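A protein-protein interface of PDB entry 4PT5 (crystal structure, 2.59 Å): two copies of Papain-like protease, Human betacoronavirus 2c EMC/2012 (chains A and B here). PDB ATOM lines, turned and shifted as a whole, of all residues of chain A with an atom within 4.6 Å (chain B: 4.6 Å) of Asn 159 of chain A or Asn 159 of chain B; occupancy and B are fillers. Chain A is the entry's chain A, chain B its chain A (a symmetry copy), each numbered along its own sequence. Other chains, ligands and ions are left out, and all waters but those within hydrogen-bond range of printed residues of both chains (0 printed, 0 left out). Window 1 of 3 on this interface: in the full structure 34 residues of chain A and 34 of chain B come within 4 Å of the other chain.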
ATOM      1  N   ARG A  84      -7.920  -7.677   5.381  1.00  0.00           N
ATOM      2  CA  ARG A  84      -8.190  -8.908   4.649  1.00  0.00           C
ATOM      3  C   ARG A  84      -9.679  -9.056   4.325  1.00  0.00           C
ATOM      4  O   ARG A  84     -10.034  -9.543   3.252  1.00  0.00           O
ATOM      5  CB  ARG A  84      -7.680 -10.097   5.461  1.00  0.00           C
ATOM      6  CG  ARG A  84      -7.394 -11.355   4.663  1.00  0.00           C
ATOM      7  CD  ARG A  84      -6.398 -12.251   5.387  1.00  0.00           C
ATOM      8  NE  ARG A  84      -6.572 -12.251   6.842  1.00  0.00           N
ATOM      9  CZ  ARG A  84      -7.393 -13.055   7.514  1.00  0.00           C
ATOM     10  NH1 ARG A  84      -8.140 -13.945   6.876  1.00  0.00           N
ATOM     11  NH2 ARG A  84      -7.469 -12.966   8.835  1.00  0.00           N
ATOM     12  N   MET A 155     -14.863 -16.329   3.947  1.00  0.00           N
ATOM     13  CA  MET A 155     -13.522 -16.377   3.378  1.00  0.00           C
ATOM     14  C   MET A 155     -12.480 -15.779   4.325  1.00  0.00           C
ATOM     15  O   MET A 155     -11.366 -16.293   4.431  1.00  0.00           O
ATOM     16  CB  MET A 155     -13.489 -15.669   2.023  1.00  0.00           C
ATOM     17  CG  MET A 155     -14.244 -16.409   0.933  1.00  0.00           C
ATOM     18  SD  MET A 155     -14.219 -15.565  -0.658  1.00  0.00           S
ATOM     19  CE  MET A 155     -12.547 -15.908  -1.202  1.00  0.00           C
ATOM     20  N   ALA A 156     -12.853 -14.703   5.018  1.00  0.00           N
ATOM     21  CA  ALA A 156     -11.965 -14.049   5.981  1.00  0.00           C
ATOM     22  C   ALA A 156     -11.671 -14.922   7.207  1.00  0.00           C
ATOM     23  O   ALA A 156     -10.511 -15.077   7.592  1.00  0.00           O
ATOM     24  CB  ALA A 156     -12.534 -12.702   6.401  1.00  0.00           C
ATOM     25  N   TYR A 157     -12.719 -15.484   7.810  1.00  0.00           N
ATOM     26  CA  TYR A 157     -12.571 -16.358   8.978  1.00  0.00           C
ATOM     27  C   TYR A 157     -11.952 -17.704   8.610  1.00  0.00           C
ATOM     28  O   TYR A 157     -11.210 -18.287   9.395  1.00  0.00           O
ATOM     29  CB  TYR A 157     -13.917 -16.593   9.666  1.00  0.00           C
ATOM     30  CG  TYR A 157     -14.417 -15.436  10.500  1.00  0.00           C
ATOM     31  CD1 TYR A 157     -13.901 -15.191  11.773  1.00  0.00           C
ATOM     32  CD2 TYR A 157     -15.428 -14.604  10.029  1.00  0.00           C
ATOM     33  CE1 TYR A 157     -14.368 -14.137  12.545  1.00  0.00           C
ATOM     34  CE2 TYR A 157     -15.900 -13.549  10.790  1.00  0.00           C
ATOM     35  CZ  TYR A 157     -15.370 -13.319  12.046  1.00  0.00           C
ATOM     36  OH  TYR A 157     -15.846 -12.268  12.797  1.00  0.00           O
ATOM     37  N   GLY A 158     -12.269 -18.193   7.415  1.00  0.00           N
ATOM     38  CA  GLY A 158     -11.688 -19.434   6.910  1.00  0.00           C
ATOM     39  C   GLY A 158     -10.287 -19.262   6.351  1.00  0.00           C
ATOM     40  O   GLY A 158      -9.636 -20.241   5.989  1.00  0.00           O
ATOM     41  N   ASN A 159      -9.823 -18.015   6.285  1.00  0.00           N
ATOM     42  CA  ASN A 159      -8.515 -17.675   5.720  1.00  0.00           C
ATOM     43  C   ASN A 159      -8.361 -18.173   4.280  1.00  0.00           C
ATOM     44  O   ASN A 159      -7.302 -18.658   3.873  1.00  0.00           O
ATOM     45  CB  ASN A 159      -7.374 -18.158   6.630  1.00  0.00           C
ATOM     46  CG  ASN A 159      -7.434 -17.542   8.019  1.00  0.00           C
ATOM     47  OD1 ASN A 159      -7.574 -16.325   8.172  1.00  0.00           O
ATOM     48  ND2 ASN A 159      -7.323 -18.382   9.043  1.00  0.00           N
ATOM     49  N   CYS A 160      -9.448 -18.049   3.525  1.00  0.00           N
ATOM     50  CA  CYS A 160      -9.469 -18.352   2.106  1.00  0.00           C
ATOM     51  C   CYS A 160      -8.903 -17.171   1.342  1.00  0.00           C
ATOM     52  O   CYS A 160      -9.167 -16.017   1.687  1.00  0.00           O
ATOM     53  CB  CYS A 160     -10.901 -18.607   1.640  1.00  0.00           C
ATOM     54  SG  CYS A 160     -11.819 -19.823   2.612  1.00  0.00           S
ATOM     55  N   THR A 161      -8.121 -17.459   0.309  1.00  0.00           N
ATOM     56  CA  THR A 161      -7.619 -16.416  -0.579  1.00  0.00           C
ATOM     57  C   THR A 161      -8.432 -16.410  -1.866  1.00  0.00           C
ATOM     58  O   THR A 161      -8.842 -17.467  -2.354  1.00  0.00           O
ATOM     59  CB  THR A 161      -6.120 -16.593  -0.903  1.00  0.00           C
ATOM     60  OG1 THR A 161      -5.894 -17.902  -1.442  1.00  0.00           O
ATOM     61  CG2 THR A 161      -5.265 -16.404   0.350  1.00  0.00           C
ATOM     62  N   ARG A 170     -13.915 -28.540   5.347  1.00  0.00           N
ATOM     63  CA  ARG A 170     -13.038 -27.712   6.165  1.00  0.00           C
ATOM     64  C   ARG A 170     -13.731 -26.410   6.520  1.00  0.00           C
ATOM     65  O   ARG A 170     -13.811 -26.030   7.695  1.00  0.00           O
ATOM     66  CB  ARG A 170     -11.766 -27.393   5.384  1.00  0.00           C
ATOM     67  CG  ARG A 170     -10.519 -27.235   6.232  1.00  0.00           C
ATOM     68  CD  ARG A 170      -9.574 -26.207   5.633  1.00  0.00           C
ATOM     69  NE  ARG A 170      -9.746 -24.909   6.275  1.00  0.00           N
ATOM     70  CZ  ARG A 170     -10.037 -23.776   5.645  1.00  0.00           C
ATOM     71  NH1 ARG A 170     -10.180 -23.748   4.327  1.00  0.00           N
ATOM     72  NH2 ARG A 170     -10.171 -22.659   6.345  1.00  0.00           N
ATOM     73  N   ARG B  84      -5.509 -32.924   7.650  1.00  0.00           N
ATOM     74  CA  ARG B  84      -4.871 -31.782   7.009  1.00  0.00           C
ATOM     75  C   ARG B  84      -3.414 -31.626   7.456  1.00  0.00           C
ATOM     76  O   ARG B  84      -2.557 -31.260   6.654  1.00  0.00           O
ATOM     77  CB  ARG B  84      -5.679 -30.521   7.310  1.00  0.00           C
ATOM     78  CG  ARG B  84      -5.489 -29.378   6.332  1.00  0.00           C
ATOM     79  CD  ARG B  84      -6.684 -28.434   6.351  1.00  0.00           C
ATOM     80  NE  ARG B  84      -7.259 -28.254   7.686  1.00  0.00           N
ATOM     81  CZ  ARG B  84      -6.857 -27.350   8.577  1.00  0.00           C
ATOM     82  NH1 ARG B  84      -5.863 -26.519   8.295  1.00  0.00           N
ATOM     83  NH2 ARG B  84      -7.452 -27.278   9.759  1.00  0.00           N
ATOM     84  N   MET B 155       1.498 -24.288   8.846  1.00  0.00           N
ATOM     85  CA  MET B 155       0.621 -24.351   7.683  1.00  0.00           C
ATOM     86  C   MET B 155      -0.773 -24.865   8.049  1.00  0.00           C
ATOM     87  O   MET B 155      -1.774 -24.378   7.523  1.00  0.00           O
ATOM     88  CB  MET B 155       1.245 -25.217   6.588  1.00  0.00           C
ATOM     89  CG  MET B 155       2.466 -24.589   5.940  1.00  0.00           C
ATOM     90  SD  MET B 155       3.211 -25.616   4.662  1.00  0.00           S
ATOM     91  CE  MET B 155       2.045 -25.395   3.321  1.00  0.00           C
ATOM     92  N   ALA B 156      -0.830 -25.838   8.958  1.00  0.00           N
ATOM     93  CA  ALA B 156      -2.100 -26.401   9.420  1.00  0.00           C
ATOM     94  C   ALA B 156      -2.938 -25.397  10.222  1.00  0.00           C
ATOM     95  O   ALA B 156      -4.129 -25.234   9.957  1.00  0.00           O
ATOM     96  CB  ALA B 156      -1.860 -27.668  10.226  1.00  0.00           C
ATOM     97  N   TYR B 157      -2.312 -24.733  11.195  1.00  0.00           N
ATOM     98  CA  TYR B 157      -2.995 -23.731  12.020  1.00  0.00           C
ATOM     99  C   TYR B 157      -3.304 -22.460  11.235  1.00  0.00           C
ATOM    100  O   TYR B 157      -4.320 -21.811  11.470  1.00  0.00           O
ATOM    101  CB  TYR B 157      -2.164 -23.373  13.254  1.00  0.00           C
ATOM    102  CG  TYR B 157      -2.184 -24.405  14.358  1.00  0.00           C
ATOM    103  CD1 TYR B 157      -3.273 -24.513  15.223  1.00  0.00           C
ATOM    104  CD2 TYR B 157      -1.099 -25.255  14.556  1.00  0.00           C
ATOM    105  CE1 TYR B 157      -3.287 -25.452  16.244  1.00  0.00           C
ATOM    106  CE2 TYR B 157      -1.104 -26.196  15.571  1.00  0.00           C
ATOM    107  CZ  TYR B 157      -2.197 -26.291  16.413  1.00  0.00           C
ATOM    108  OH  TYR B 157      -2.192 -27.229  17.421  1.00  0.00           O
ATOM    109  N   GLY B 158      -2.419 -22.107  10.309  1.00  0.00           N
ATOM    110  CA  GLY B 158      -2.630 -20.954   9.437  1.00  0.00           C
ATOM    111  C   GLY B 158      -3.571 -21.237   8.279  1.00  0.00           C
ATOM    112  O   GLY B 158      -3.923 -20.329   7.527  1.00  0.00           O
ATOM    113  N   ASN B 159      -3.980 -22.497   8.140  1.00  0.00           N
ATOM    114  CA  ASN B 159      -4.843 -22.944   7.043  1.00  0.00           C
ATOM    115  C   ASN B 159      -4.242 -22.626   5.671  1.00  0.00           C
ATOM    116  O   ASN B 159      -4.942 -22.228   4.735  1.00  0.00           O
ATOM    117  CB  ASN B 159      -6.269 -22.393   7.198  1.00  0.00           C
ATOM    118  CG  ASN B 159      -6.929 -22.836   8.494  1.00  0.00           C
ATOM    119  OD1 ASN B 159      -6.923 -24.020   8.841  1.00  0.00           O
ATOM    120  ND2 ASN B 159      -7.509 -21.883   9.219  1.00  0.00           N
ATOM    121  N   CYS B 160      -2.928 -22.805   5.579  1.00  0.00           N
ATOM    122  CA  CYS B 160      -2.193 -22.673   4.335  1.00  0.00           C
ATOM    123  C   CYS B 160      -2.340 -23.955   3.538  1.00  0.00           C
ATOM    124  O   CYS B 160      -2.320 -25.050   4.103  1.00  0.00           O
ATOM    125  CB  CYS B 160      -0.711 -22.430   4.618  1.00  0.00           C
ATOM    126  SG  CYS B 160      -0.362 -21.078   5.765  1.00  0.00           S
ATOM    127  N   THR B 161      -2.493 -23.817   2.227  1.00  0.00           N
ATOM    128  CA  THR B 161      -2.520 -24.975   1.339  1.00  0.00           C
ATOM    129  C   THR B 161      -1.174 -25.108   0.640  1.00  0.00           C
ATOM    130  O   THR B 161      -0.542 -24.105   0.299  1.00  0.00           O
ATOM    131  CB  THR B 161      -3.651 -24.886   0.292  1.00  0.00           C
ATOM    132  OG1 THR B 161      -3.536 -23.658  -0.440  1.00  0.00           O
ATOM    133  CG2 THR B 161      -5.022 -24.951   0.965  1.00  0.00           C
ATOM    134  N   ARG B 170       0.370 -12.034   8.116  1.00  0.00           N
ATOM    135  CA  ARG B 170      -0.824 -12.786   8.481  1.00  0.00           C
ATOM    136  C   ARG B 170      -0.442 -14.013   9.287  1.00  0.00           C
ATOM    137  O   ARG B 170      -0.971 -14.247  10.381  1.00  0.00           O
ATOM    138  CB  ARG B 170      -1.547 -13.236   7.214  1.00  0.00           C
ATOM    139  CG  ARG B 170      -3.055 -13.332   7.340  1.00  0.00           C
ATOM    140  CD  ARG B 170      -3.608 -14.454   6.477  1.00  0.00           C
ATOM    141  NE  ARG B 170      -3.821 -15.660   7.269  1.00  0.00           N
ATOM    142  CZ  ARG B 170      -3.291 -16.850   7.009  1.00  0.00           C
ATOM    143  NH1 ARG B 170      -2.511 -17.031   5.952  1.00  0.00           N
ATOM    144  NH2 ARG B 170      -3.559 -17.871   7.810  1.00  0.00           N
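Arg 84 of chain A touches Arg 170 of chain B, and with the chains exchanged Arg 170 of chain A touches Arg 84 of chain B. Asn 159 of chain B touches its own counterpart, Asn 159 of chain A. Asn 159 of chain A touches Arg 170 of chain B, and with the chains exchanged Arg 170 of chain A touches Asn 159 of chain B. Positions printed for both chains: 84, 155, 156, 157, 158, 159, 160, 161 and 170. Of the 5 pairs that touch across the chains among the printed residues, 5 have their exchanged pair printed and touching as well.
Of chain B, only Asn 159 and Arg 170 come within 4 Å of Asn 159 of chain A. Of chain A, only Asn 159 and Arg 170 come within 4 Å of Asn 159 of chain B. Printed residues of chain B within 4 Å of Arg 84 of chain A: Arg 170 (3.7 Å). Of the printed residues of chain A, Arg 170 of chain B touches Arg 84 (3.7 Å) and Asn 159 (3.9 Å). Thr 161 of chain A touches none of the printed residues of chain B. Gly 158 of chain B touches none of the printed residues of chain A. The nearest residue of chain B that does not touch Asn 159 of chain A is Gly 158 of chain B (4.2 Å). The nearest printed residue of chain A that does not touch Arg 170 of chain B is Thr 161 of chain A (6.3 Å).
O of Ala 156 of chain A sits at hydrogen-bond distance from NH1 of Arg 84 of chain A, 2.7 Å away. The backbone carbonyl oxygen (O) of Ala 156 of chain A sits close to the side-chain amide oxygen (OD1) of Asn 159 of chain A, 3.2 Å away. O of Ala 156 of chain B is in hydrogen-bond range of NH1 of Arg 84 of chain B (2.7 Å). The guanidinium group of Arg 84 of chain B lies within hydrogen-bond range of the side-chain amide oxygen of Asn 159 of chain B, 2.8 Å away. The backbone carbonyl oxygen (O) of Ala 156 of chain B lies close to the side-chain amide oxygen (OD1) of Asn 159 of chain B (3.2 Å). NH2 of Arg 170 of chain B sits at hydrogen-bond distance from O of Gly 158 of chain B, at 2.5 Å.
Of the 9 printed residues of chain A, 3 touch a printed residue of chain B. Of the 9 printed residues of chain B, 3 touch a printed residue of chain A.
Arg 170 of chain B touches Arg 84 of chain A (CD to NE, 3.7 Å). Asn 159 of chain B touches Asn 159 of chain A (ND2 to ND2, 3.5 Å). CG of Asn 159 of chain A touches NH2 of Arg 170 of chain B (3.9 Å). Arg 170 of chain A touches Arg 84 of chain B (CD to NE, 3.7 Å). Asn 159 of chain B touches Arg 170 of chain A (CG to NH2, 3.9 Å).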
